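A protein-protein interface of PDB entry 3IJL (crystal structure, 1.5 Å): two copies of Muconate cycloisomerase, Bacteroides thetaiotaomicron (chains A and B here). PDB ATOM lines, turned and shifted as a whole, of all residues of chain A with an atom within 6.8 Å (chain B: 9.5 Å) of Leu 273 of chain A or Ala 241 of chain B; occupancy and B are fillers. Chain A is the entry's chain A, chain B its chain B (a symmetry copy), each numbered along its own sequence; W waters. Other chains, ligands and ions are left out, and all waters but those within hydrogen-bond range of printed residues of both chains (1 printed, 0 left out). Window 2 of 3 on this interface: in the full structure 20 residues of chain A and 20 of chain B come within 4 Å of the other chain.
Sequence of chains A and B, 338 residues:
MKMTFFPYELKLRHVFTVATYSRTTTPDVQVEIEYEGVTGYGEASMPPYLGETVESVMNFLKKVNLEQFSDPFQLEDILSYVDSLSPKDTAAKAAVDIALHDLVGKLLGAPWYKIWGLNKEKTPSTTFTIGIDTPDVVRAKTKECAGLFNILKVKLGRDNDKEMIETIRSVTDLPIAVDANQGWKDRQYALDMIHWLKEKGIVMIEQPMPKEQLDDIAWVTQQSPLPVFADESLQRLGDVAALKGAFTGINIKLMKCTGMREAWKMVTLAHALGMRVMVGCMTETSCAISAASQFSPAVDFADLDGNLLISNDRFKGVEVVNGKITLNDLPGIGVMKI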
ATOM      1  N   VAL A 240       4.444 -10.751 -17.310  1.00  0.00           N
ATOM      2  CA  VAL A 240       4.992  -9.717 -16.440  1.00  0.00           C
ATOM      3  C   VAL A 240       5.667  -8.513 -17.100  1.00  0.00           C
ATOM      4  O   VAL A 240       5.306  -7.368 -16.827  1.00  0.00           O
ATOM      5  CB  VAL A 240       5.994 -10.331 -15.445  1.00  0.00           C
ATOM      6  CG1 VAL A 240       6.551  -9.252 -14.532  1.00  0.00           C
ATOM      7  CG2 VAL A 240       5.313 -11.421 -14.631  1.00  0.00           C
ATOM      8  N   ALA A 241       6.653  -8.775 -17.951  1.00  0.00           N
ATOM      9  CA  ALA A 241       7.406  -7.712 -18.614  1.00  0.00           C
ATOM     10  C   ALA A 241       6.558  -6.616 -19.254  1.00  0.00           C
ATOM     11  O   ALA A 241       6.884  -5.434 -19.153  1.00  0.00           O
ATOM     12  CB  ALA A 241       8.342  -8.319 -19.655  1.00  0.00           C
ATOM     13  N   ALA A 242       5.471  -7.009 -19.908  1.00  0.00           N
ATOM     14  CA  ALA A 242       4.595  -6.053 -20.577  1.00  0.00           C
ATOM     15  C   ALA A 242       3.970  -5.025 -19.636  1.00  0.00           C
ATOM     16  O   ALA A 242       3.480  -3.987 -20.081  1.00  0.00           O
ATOM     17  CB  ALA A 242       3.499  -6.800 -21.323  1.00  0.00           C
ATOM     18  N   LYS A 244       5.635  -3.483 -17.079  1.00  0.00           N
ATOM     19  CA  LYS A 244       6.617  -2.547 -16.550  1.00  0.00           C
ATOM     20  C   LYS A 244       6.245  -1.128 -16.970  1.00  0.00           C
ATOM     21  O   LYS A 244       5.941  -0.879 -18.136  1.00  0.00           O
ATOM     22  CB  LYS A 244       8.014  -2.889 -17.076  1.00  0.00           C
ATOM     23  CG  LYS A 244       9.124  -2.026 -16.499  1.00  0.00           C
ATOM     24  CD  LYS A 244      10.482  -2.416 -17.066  1.00  0.00           C
ATOM     25  CE  LYS A 244      11.609  -1.673 -16.365  1.00  0.00           C
ATOM     26  NZ  LYS A 244      11.485  -0.196 -16.503  1.00  0.00           N
ATOM     27  N   GLY A 245       6.259  -0.203 -16.015  1.00  0.00           N
ATOM     28  CA  GLY A 245       5.925   1.177 -16.322  1.00  0.00           C
ATOM     29  C   GLY A 245       4.446   1.510 -16.248  1.00  0.00           C
ATOM     30  O   GLY A 245       4.072   2.683 -16.193  1.00  0.00           O
ATOM     31  N   VAL A 267       8.750 -13.498  -9.055  1.00  0.00           N
ATOM     32  CA  VAL A 267       9.238 -12.576  -8.035  1.00  0.00           C
ATOM     33  C   VAL A 267      10.568 -12.009  -8.520  1.00  0.00           C
ATOM     34  O   VAL A 267      10.804 -10.803  -8.449  1.00  0.00           O
ATOM     35  CB  VAL A 267       9.472 -13.285  -6.681  1.00  0.00           C
ATOM     36  CG1 VAL A 267      10.145 -12.327  -5.701  1.00  0.00           C
ATOM     37  CG2 VAL A 267       8.152 -13.774  -6.114  1.00  0.00           C
ATOM     38  N   THR A 268      11.432 -12.893  -9.015  1.00  0.00           N
ATOM     39  CA  THR A 268      12.742 -12.492  -9.519  1.00  0.00           C
ATOM     40  C   THR A 268      12.606 -11.512 -10.677  1.00  0.00           C
ATOM     41  O   THR A 268      13.261 -10.468 -10.703  1.00  0.00           O
ATOM     42  CB  THR A 268      13.554 -13.717 -10.008  1.00  0.00           C
ATOM     43  OG1 THR A 268      13.820 -14.588  -8.902  1.00  0.00           O
ATOM     44  CG2 THR A 268      14.873 -13.275 -10.628  1.00  0.00           C
ATOM     45  N   LEU A 269      11.754 -11.855 -11.637  1.00  0.00           N
ATOM     46  CA  LEU A 269      11.537 -11.013 -12.805  1.00  0.00           C
ATOM     47  C   LEU A 269      10.997  -9.638 -12.422  1.00  0.00           C
ATOM     48  O   LEU A 269      11.540  -8.611 -12.829  1.00  0.00           O
ATOM     49  CB  LEU A 269      10.573 -11.700 -13.777  1.00  0.00           C
ATOM     50  CG  LEU A 269      10.218 -10.923 -15.049  1.00  0.00           C
ATOM     51  CD1 LEU A 269      11.490 -10.573 -15.804  1.00  0.00           C
ATOM     52  CD2 LEU A 269       9.295 -11.751 -15.927  1.00  0.00           C
ATOM     53  N   ALA A 270       9.928  -9.620 -11.631  1.00  0.00           N
ATOM     54  CA  ALA A 270       9.336  -8.359 -11.208  1.00  0.00           C
ATOM     55  C   ALA A 270      10.373  -7.463 -10.532  1.00  0.00           C
ATOM     56  O   ALA A 270      10.533  -6.300 -10.905  1.00  0.00           O
ATOM     57  CB  ALA A 270       8.162  -8.622 -10.259  1.00  0.00           C
ATOM     58  N   HIS A 271      11.076  -8.011  -9.544  1.00  0.00           N
ATOM     59  CA  HIS A 271      12.095  -7.261  -8.813  1.00  0.00           C
ATOM     60  C   HIS A 271      13.232  -6.779  -9.702  1.00  0.00           C
ATOM     61  O   HIS A 271      13.701  -5.646  -9.561  1.00  0.00           O
ATOM     62  CB  HIS A 271      12.660  -8.113  -7.676  1.00  0.00           C
ATOM     63  CG  HIS A 271      11.765  -8.189  -6.479  1.00  0.00           C
ATOM     64  ND1 HIS A 271      11.982  -9.072  -5.444  1.00  0.00           N
ATOM     65  CD2 HIS A 271      10.668  -7.470  -6.137  1.00  0.00           C
ATOM     66  CE1 HIS A 271      11.058  -8.893  -4.516  1.00  0.00           C
ATOM     67  NE2 HIS A 271      10.249  -7.927  -4.911  1.00  0.00           N
ATOM     68  N   ALA A 272      13.677  -7.634 -10.616  1.00  0.00           N
ATOM     69  CA  ALA A 272      14.762  -7.267 -11.517  1.00  0.00           C
ATOM     70  C   ALA A 272      14.338  -6.081 -12.373  1.00  0.00           C
ATOM     71  O   ALA A 272      15.164  -5.244 -12.743  1.00  0.00           O
ATOM     72  CB  ALA A 272      15.135  -8.452 -12.403  1.00  0.00           C
ATOM     73  N   LEU A 273      13.045  -6.009 -12.674  1.00  0.00           N
ATOM     74  CA  LEU A 273      12.494  -4.930 -13.489  1.00  0.00           C
ATOM     75  C   LEU A 273      12.039  -3.719 -12.669  1.00  0.00           C
ATOM     76  O   LEU A 273      11.389  -2.818 -13.197  1.00  0.00           O
ATOM     77  CB  LEU A 273      11.317  -5.444 -14.321  1.00  0.00           C
ATOM     78  CG  LEU A 273      11.611  -6.556 -15.332  1.00  0.00           C
ATOM     79  CD1 LEU A 273      10.332  -6.915 -16.075  1.00  0.00           C
ATOM     80  CD2 LEU A 273      12.684  -6.096 -16.312  1.00  0.00           C
ATOM     81  N   GLY A 274      12.373  -3.707 -11.383  1.00  0.00           N
ATOM     82  CA  GLY A 274      11.998  -2.590 -10.531  1.00  0.00           C
ATOM     83  C   GLY A 274      10.541  -2.552 -10.105  1.00  0.00           C
ATOM     84  O   GLY A 274      10.046  -1.508  -9.676  1.00  0.00           O
ATOM     85  N   MET A 275       9.847  -3.680 -10.219  1.00  0.00           N
ATOM     86  CA  MET A 275       8.443  -3.754  -9.828  1.00  0.00           C
ATOM     87  C   MET A 275       8.316  -4.417  -8.464  1.00  0.00           C
ATOM     88  O   MET A 275       9.160  -5.227  -8.080  1.00  0.00           O
ATOM     89  CB  MET A 275       7.642  -4.566 -10.847  1.00  0.00           C
ATOM     90  CG  MET A 275       7.644  -4.000 -12.252  1.00  0.00           C
ATOM     91  SD  MET A 275       6.729  -5.064 -13.391  1.00  0.00           S
ATOM     92  CE  MET A 275       5.100  -4.429 -13.199  1.00  0.00           C
ATOM     93  N   LEU B 214      24.986   0.032 -28.989  1.00  0.00           N
ATOM     94  CA  LEU B 214      23.903  -0.932 -28.837  1.00  0.00           C
ATOM     95  C   LEU B 214      22.986  -0.896 -30.052  1.00  0.00           C
ATOM     96  O   LEU B 214      22.457  -1.922 -30.476  1.00  0.00           O
ATOM     97  CB  LEU B 214      23.095  -0.623 -27.573  1.00  0.00           C
ATOM     98  CG  LEU B 214      21.980  -1.612 -27.223  1.00  0.00           C
ATOM     99  CD1 LEU B 214      22.579  -2.983 -26.944  1.00  0.00           C
ATOM    100  CD2 LEU B 214      21.213  -1.111 -26.009  1.00  0.00           C
ATOM    101  N   SER B 233      28.903  -5.866 -22.648  1.00  0.00           N
ATOM    102  CA  SER B 233      27.687  -5.063 -22.568  1.00  0.00           C
ATOM    103  C   SER B 233      26.914  -5.225 -21.259  1.00  0.00           C
ATOM    104  O   SER B 233      25.908  -4.546 -21.050  1.00  0.00           O
ATOM    105  CB  SER B 233      26.756  -5.371 -23.747  1.00  0.00           C
ATOM    106  OG  SER B 233      27.148  -4.650 -24.906  1.00  0.00           O
ATOM    107  N   LEU B 234      27.359  -6.122 -20.381  1.00  0.00           N
ATOM    108  CA  LEU B 234      26.673  -6.294 -19.098  1.00  0.00           C
ATOM    109  C   LEU B 234      27.575  -6.878 -18.024  1.00  0.00           C
ATOM    110  O   LEU B 234      28.561  -7.551 -18.317  1.00  0.00           O
ATOM    111  CB  LEU B 234      25.434  -7.193 -19.235  1.00  0.00           C
ATOM    112  CG  LEU B 234      25.636  -8.715 -19.172  1.00  0.00           C
ATOM    113  CD1 LEU B 234      24.322  -9.400 -18.810  1.00  0.00           C
ATOM    114  CD2 LEU B 234      26.163  -9.229 -20.503  1.00  0.00           C
ATOM    115  N   GLN B 235      27.229  -6.608 -16.770  1.00  0.00           N
ATOM    116  CA  GLN B 235      27.987  -7.139 -15.650  1.00  0.00           C
ATOM    117  C   GLN B 235      27.055  -7.801 -14.652  1.00  0.00           C
ATOM    118  O   GLN B 235      27.272  -8.944 -14.246  1.00  0.00           O
ATOM    119  CB  GLN B 235      28.751  -6.027 -14.932  1.00  0.00           C
ATOM    120  CG  GLN B 235      29.773  -5.311 -15.790  1.00  0.00           C
ATOM    121  CD  GLN B 235      30.535  -4.268 -15.006  1.00  0.00           C
ATOM    122  OE1 GLN B 235      29.941  -3.483 -14.271  1.00  0.00           O
ATOM    123  NE2 GLN B 235      31.854  -4.251 -15.160  1.00  0.00           N
ATOM    124  N   ARG B 236      26.006  -7.077 -14.276  1.00  0.00           N
ATOM    125  CA  ARG B 236      25.065  -7.554 -13.275  1.00  0.00           C
ATOM    126  C   ARG B 236      23.608  -7.641 -13.713  1.00  0.00           C
ATOM    127  O   ARG B 236      23.256  -7.301 -14.843  1.00  0.00           O
ATOM    128  CB  ARG B 236      25.185  -6.673 -12.031  1.00  0.00           C
ATOM    129  CG  ARG B 236      26.600  -6.633 -11.474  1.00  0.00           C
ATOM    130  CD  ARG B 236      26.656  -5.924 -10.134  1.00  0.00           C
ATOM    131  NE  ARG B 236      25.802  -6.587  -9.154  1.00  0.00           N
ATOM    132  CZ  ARG B 236      25.767  -6.281  -7.865  1.00  0.00           C
ATOM    133  NH1 ARG B 236      26.543  -5.313  -7.390  1.00  0.00           N
ATOM    134  NH2 ARG B 236      24.956  -6.941  -7.049  1.00  0.00           N
ATOM    135  N   LEU B 237      22.766  -8.098 -12.789  1.00  0.00           N
ATOM    136  CA  LEU B 237      21.342  -8.277 -13.042  1.00  0.00           C
ATOM    137  C   LEU B 237      20.667  -7.045 -13.639  1.00  0.00           C
ATOM    138  O   LEU B 237      19.875  -7.151 -14.579  1.00  0.00           O
ATOM    139  CB  LEU B 237      20.643  -8.668 -11.740  1.00  0.00           C
ATOM    140  CG  LEU B 237      19.182  -9.113 -11.835  1.00  0.00           C
ATOM    141  CD1 LEU B 237      19.087 -10.385 -12.670  1.00  0.00           C
ATOM    142  CD2 LEU B 237      18.635  -9.352 -10.438  1.00  0.00           C
ATOM    143  N   GLY B 238      20.998  -5.878 -13.097  1.00  0.00           N
ATOM    144  CA  GLY B 238      20.401  -4.640 -13.568  1.00  0.00           C
ATOM    145  C   GLY B 238      20.789  -4.201 -14.967  1.00  0.00           C
ATOM    146  O   GLY B 238      20.249  -3.220 -15.476  1.00  0.00           O
ATOM    147  N   ASP B 239      21.716  -4.918 -15.597  1.00  0.00           N
ATOM    148  CA  ASP B 239      22.159  -4.572 -16.947  1.00  0.00           C
ATOM    149  C   ASP B 239      21.511  -5.430 -18.034  1.00  0.00           C
ATOM    150  O   ASP B 239      21.652  -5.147 -19.223  1.00  0.00           O
ATOM    151  CB  ASP B 239      23.680  -4.735 -17.081  1.00  0.00           C
ATOM    152  CG  ASP B 239      24.459  -3.960 -16.038  1.00  0.00           C
ATOM    153  OD1 ASP B 239      24.021  -2.857 -15.654  1.00  0.00           O
ATOM    154  OD2 ASP B 239      25.529  -4.449 -15.620  1.00  0.00           O
ATOM    155  N   VAL B 240      20.801  -6.474 -17.626  1.00  0.00           N
ATOM    156  CA  VAL B 240      20.192  -7.409 -18.569  1.00  0.00           C
ATOM    157  C   VAL B 240      19.031  -6.916 -19.432  1.00  0.00           C
ATOM    158  O   VAL B 240      19.061  -7.054 -20.658  1.00  0.00           O
ATOM    159  CB  VAL B 240      19.725  -8.686 -17.832  1.00  0.00           C
ATOM    160  CG1 VAL B 240      19.082  -9.656 -18.817  1.00  0.00           C
ATOM    161  CG2 VAL B 240      20.907  -9.341 -17.134  1.00  0.00           C
ATOM    162  N   ALA B 241      18.013  -6.348 -18.797  1.00  0.00           N
ATOM    163  CA  ALA B 241      16.822  -5.883 -19.505  1.00  0.00           C
ATOM    164  C   ALA B 241      17.076  -4.975 -20.702  1.00  0.00           C
ATOM    165  O   ALA B 241      16.412  -5.101 -21.731  1.00  0.00           O
ATOM    166  CB  ALA B 241      15.886  -5.193 -18.527  1.00  0.00           C
ATOM    167  N   ALA B 242      18.031  -4.064 -20.569  1.00  0.00           N
ATOM    168  CA  ALA B 242      18.344  -3.126 -21.642  1.00  0.00           C
ATOM    169  C   ALA B 242      18.845  -3.798 -22.916  1.00  0.00           C
ATOM    170  O   ALA B 242      18.850  -3.186 -23.987  1.00  0.00           O
ATOM    171  CB  ALA B 242      19.374  -2.112 -21.156  1.00  0.00           C
ATOM    172  N   LEU B 243      19.257  -5.057 -22.808  1.00  0.00           N
ATOM    173  CA  LEU B 243      19.783  -5.776 -23.961  1.00  0.00           C
ATOM    174  C   LEU B 243      18.739  -6.559 -24.749  1.00  0.00           C
ATOM    175  O   LEU B 243      19.034  -7.081 -25.824  1.00  0.00           O
ATOM    176  CB  LEU B 243      20.903  -6.715 -23.507  1.00  0.00           C
ATOM    177  CG  LEU B 243      22.001  -6.036 -22.683  1.00  0.00           C
ATOM    178  CD1 LEU B 243      23.042  -7.068 -22.279  1.00  0.00           C
ATOM    179  CD2 LEU B 243      22.643  -4.913 -23.490  1.00  0.00           C
ATOM    180  N   LYS B 244      17.524  -6.647 -24.218  1.00  0.00           N
ATOM    181  CA  LYS B 244      16.464  -7.369 -24.909  1.00  0.00           C
ATOM    182  C   LYS B 244      16.221  -6.732 -26.272  1.00  0.00           C
ATOM    183  O   LYS B 244      16.043  -5.518 -26.376  1.00  0.00           O
ATOM    184  CB  LYS B 244      15.171  -7.340 -24.089  1.00  0.00           C
ATOM    185  CG  LYS B 244      13.983  -7.983 -24.793  1.00  0.00           C
ATOM    186  CD  LYS B 244      12.719  -7.894 -23.953  1.00  0.00           C
ATOM    187  CE  LYS B 244      11.521  -8.460 -24.702  1.00  0.00           C
ATOM    188  NZ  LYS B 244      11.731  -9.882 -25.100  1.00  0.00           N
ATOM    189  N   GLY B 245      16.229  -7.553 -27.317  1.00  0.00           N
ATOM    190  CA  GLY B 245      16.003  -7.039 -28.656  1.00  0.00           C
ATOM    191  C   GLY B 245      17.266  -6.645 -29.400  1.00  0.00           C
ATOM    192  O   GLY B 245      17.237  -6.472 -30.619  1.00  0.00           O
ATOM    193  N   ALA B 246      18.375  -6.505 -28.678  1.00  0.00           N
ATOM    194  CA  ALA B 246      19.643  -6.125 -29.290  1.00  0.00           C
ATOM    195  C   ALA B 246      20.593  -7.314 -29.394  1.00  0.00           C
ATOM    196  O   ALA B 246      21.393  -7.404 -30.327  1.00  0.00           O
ATOM    197  CB  ALA B 246      20.297  -5.012 -28.484  1.00  0.00           C
ATOM    198  N   PHE B 247      20.498  -8.216 -28.423  1.00  0.00           N
ATOM    199  CA  PHE B 247      21.337  -9.411 -28.363  1.00  0.00           C
ATOM    200  C   PHE B 247      20.486 -10.673 -28.322  1.00  0.00           C
ATOM    201  O   PHE B 247      19.362 -10.657 -27.820  1.00  0.00           O
ATOM    202  CB  PHE B 247      22.200  -9.382 -27.100  1.00  0.00           C
ATOM    203  CG  PHE B 247      23.397  -8.489 -27.191  1.00  0.00           C
ATOM    204  CD1 PHE B 247      24.590  -8.959 -27.730  1.00  0.00           C
ATOM    205  CD2 PHE B 247      23.352  -7.190 -26.693  1.00  0.00           C
ATOM    206  CE1 PHE B 247      25.725  -8.154 -27.767  1.00  0.00           C
ATOM    207  CE2 PHE B 247      24.479  -6.375 -26.726  1.00  0.00           C
ATOM    208  CZ  PHE B 247      25.670  -6.860 -27.262  1.00  0.00           C
ATOM    209  N   ILE B 250      22.838 -13.470 -23.307  1.00  0.00           N
ATOM    210  CA  ILE B 250      23.828 -12.840 -22.446  1.00  0.00           C
ATOM    211  C   ILE B 250      24.850 -13.840 -21.934  1.00  0.00           C
ATOM    212  O   ILE B 250      24.574 -15.033 -21.845  1.00  0.00           O
ATOM    213  CB  ILE B 250      23.170 -12.180 -21.210  1.00  0.00           C
ATOM    214  CG1 ILE B 250      22.461 -13.238 -20.358  1.00  0.00           C
ATOM    215  CG2 ILE B 250      22.175 -11.113 -21.651  1.00  0.00           C
ATOM    216  CD1 ILE B 250      22.002 -12.719 -19.001  1.00  0.00           C
ATOM    217  N   LYS B 265      19.762 -15.570 -10.902  1.00  0.00           N
ATOM    218  CA  LYS B 265      18.694 -14.612 -11.163  1.00  0.00           C
ATOM    219  C   LYS B 265      18.834 -14.077 -12.586  1.00  0.00           C
ATOM    220  O   LYS B 265      17.839 -13.788 -13.250  1.00  0.00           O
ATOM    221  CB  LYS B 265      18.746 -13.453 -10.168  1.00  0.00           C
ATOM    222  CG  LYS B 265      18.302 -13.822  -8.766  1.00  0.00           C
ATOM    223  CD  LYS B 265      18.413 -12.613  -7.854  1.00  0.00           C
ATOM    224  CE  LYS B 265      18.073 -12.954  -6.426  1.00  0.00           C
ATOM    225  NZ  LYS B 265      18.179 -11.749  -5.557  1.00  0.00           N
ATOM    226  N   MET B 266      20.074 -13.939 -13.051  1.00  0.00           N
ATOM    227  CA  MET B 266      20.321 -13.450 -14.403  1.00  0.00           C
ATOM    228  C   MET B 266      19.866 -14.479 -15.435  1.00  0.00           C
ATOM    229  O   MET B 266      19.347 -14.121 -16.495  1.00  0.00           O
ATOM    230  CB  MET B 266      21.804 -13.120 -14.584  1.00  0.00           C
ATOM    231  CG  MET B 266      22.224 -11.874 -13.826  1.00  0.00           C
ATOM    232  SD  MET B 266      24.003 -11.598 -13.802  1.00  0.00           S
ATOM    233  CE  MET B 266      24.274 -10.900 -15.431  1.00  0.00           C
ATOM    234  N   THR B 268      17.459 -16.646 -14.986  1.00  0.00           N
ATOM    235  CA  THR B 268      16.006 -16.570 -14.921  1.00  0.00           C
ATOM    236  C   THR B 268      15.488 -15.359 -15.689  1.00  0.00           C
ATOM    237  O   THR B 268      14.552 -15.466 -16.483  1.00  0.00           O
ATOM    238  CB  THR B 268      15.523 -16.475 -13.448  1.00  0.00           C
ATOM    239  OG1 THR B 268      15.905 -17.665 -12.746  1.00  0.00           O
ATOM    240  CG2 THR B 268      14.014 -16.316 -13.383  1.00  0.00           C
ATOM    241  N   LEU B 269      16.107 -14.206 -15.457  1.00  0.00           N
ATOM    242  CA  LEU B 269      15.694 -12.979 -16.123  1.00  0.00           C
ATOM    243  C   LEU B 269      15.853 -13.071 -17.635  1.00  0.00           C
ATOM    244  O   LEU B 269      14.921 -12.783 -18.386  1.00  0.00           O
ATOM    245  CB  LEU B 269      16.496 -11.786 -15.585  1.00  0.00           C
ATOM    246  CG  LEU B 269      16.218 -10.422 -16.223  1.00  0.00           C
ATOM    247  CD1 LEU B 269      14.741 -10.078 -16.106  1.00  0.00           C
ATOM    248  CD2 LEU B 269      17.053  -9.357 -15.531  1.00  0.00           C
ATOM    249  N   ALA B 270      17.033 -13.478 -18.086  1.00  0.00           N
ATOM    250  CA  ALA B 270      17.281 -13.592 -19.514  1.00  0.00           C
ATOM    251  C   ALA B 270      16.261 -14.520 -20.172  1.00  0.00           C
ATOM    252  O   ALA B 270      15.653 -14.164 -21.182  1.00  0.00           O
ATOM    253  CB  ALA B 270      18.694 -14.106 -19.758  1.00  0.00           C
ATOM    254  N   ALA B 272      13.312 -15.452 -19.096  1.00  0.00           N
ATOM    255  CA  ALA B 272      11.971 -14.888 -19.003  1.00  0.00           C
ATOM    256  C   ALA B 272      11.762 -13.843 -20.093  1.00  0.00           C
ATOM    257  O   ALA B 272      10.647 -13.664 -20.583  1.00  0.00           O
ATOM    258  CB  ALA B 272      11.756 -14.265 -17.624  1.00  0.00           C
ATOM    259  N   LEU B 273      12.839 -13.159 -20.474  1.00  0.00           N
ATOM    260  CA  LEU B 273      12.772 -12.130 -21.508  1.00  0.00           C
ATOM    261  C   LEU B 273      13.020 -12.690 -22.909  1.00  0.00           C
ATOM    262  O   LEU B 273      13.203 -11.933 -23.865  1.00  0.00           O
ATOM    263  CB  LEU B 273      13.781 -11.017 -21.213  1.00  0.00           C
ATOM    264  CG  LEU B 273      13.545 -10.195 -19.942  1.00  0.00           C
ATOM    265  CD1 LEU B 273      14.638  -9.144 -19.804  1.00  0.00           C
ATOM    266  CD2 LEU B 273      12.170  -9.529 -20.007  1.00  0.00           C
ATOM    267  N   MET B 275      15.631 -14.359 -23.973  1.00  0.00           N
ATOM    268  CA  MET B 275      17.035 -14.315 -24.374  1.00  0.00           C
ATOM    269  C   MET B 275      17.736 -15.614 -24.007  1.00  0.00           C
ATOM    270  O   MET B 275      17.325 -16.307 -23.079  1.00  0.00           O
ATOM    271  CB  MET B 275      17.757 -13.159 -23.680  1.00  0.00           C
ATOM    272  CG  MET B 275      17.258 -11.777 -24.061  1.00  0.00           C
ATOM    273  SD  MET B 275      18.129 -10.491 -23.133  1.00  0.00           S
ATOM    274  CE  MET B 275      19.504 -10.201 -24.185  1.00  0.00           C
HETATM  275  O   HOH W   1      15.153 -16.616 -10.189  1.00  0.00           O
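Lys 265 of chain B touches Thr 268 of chain A (CB to CG2, 3.9 Å). CD1 of Leu 269 of chain B touches CD1 of Leu 269 of chain A, at 3.3 Å. Leu 269 of chain A touches Ala 272 of chain B. CB of Ala 272 of chain A touches CD2 of Leu 269 of chain B, at 3.8 Å. Leu 273 of chain A touches Ala 241 of chain B.
Printed residues of chain B within 4 Å of Leu 273 of chain A: Ala 241. Of the printed residues of chain A, Ala 241 of chain B touches Leu 273 (3.997 Å). No residue of chain B comes within 4 Å of Ala 241 of chain A. Ala 272 of chain A touches just one residue of chain B: Leu 269. No residue of chain B comes within 4 Å of Gly 274 of chain A. Of the printed residues of chain A, Leu 269 of chain B touches Leu 269 (3.3 Å) and Ala 272 (3.8 Å). Of the printed residues of chain B, Thr 268 of chain A touches Lys 265. Of the printed residues of chain A, Ala 272 of chain B touches Leu 269. Leu 243 of chain B touches none of the printed residues of chain A. The nearest printed residue of chain A that does not touch Ala 241 of chain B is Ala 272 of chain A (5.8 Å). The nearest printed residue of chain A that does not touch Lys 265 of chain B is Ala 272 of chain A (6.0 Å).
Printed residues of chain A that touch a printed residue of chain B: Thr 268, Leu 269, Ala 272 and Leu 273. Hydrophobic or aromatic side chains of chain A that line the printed part of chain B: Leu 269, Ala 272 and Leu 273. Printed residues of chain B that touch a printed residue of chain A: Ala 241, Lys 265, Leu 269 and Ala 272. Hydrophobic or aromatic side chains of chain B that line the printed part of chain A: Ala 241, Leu 269 and Ala 272. Among the printed residues, no Asp or Glu carboxylate lies within 4 Å of a Lys or Arg side-chain nitrogen of the other chain.
Leu 269 of chain B touches its own counterpart, Leu 269 of chain A. Leu 269 of chain A touches Ala 272 of chain B, and with the chains exchanged Ala 272 of chain A touches Leu 269 of chain B. Leu 273 of chain A touches Ala 241 of chain B, but with the chains exchanged Ala 241 of chain A does not touch Leu 273 of chain B (4.03 Å). Positions printed for both chains: 240, 241, 242, 244, 245, 268, 269, 270, 272, 273 and 275.
Water W1 bridges the side-chain hydroxyl of Thr 268 of chain A (2.7 Å) and the side-chain hydroxyl of Thr 268 of chain B (2.9 Å).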
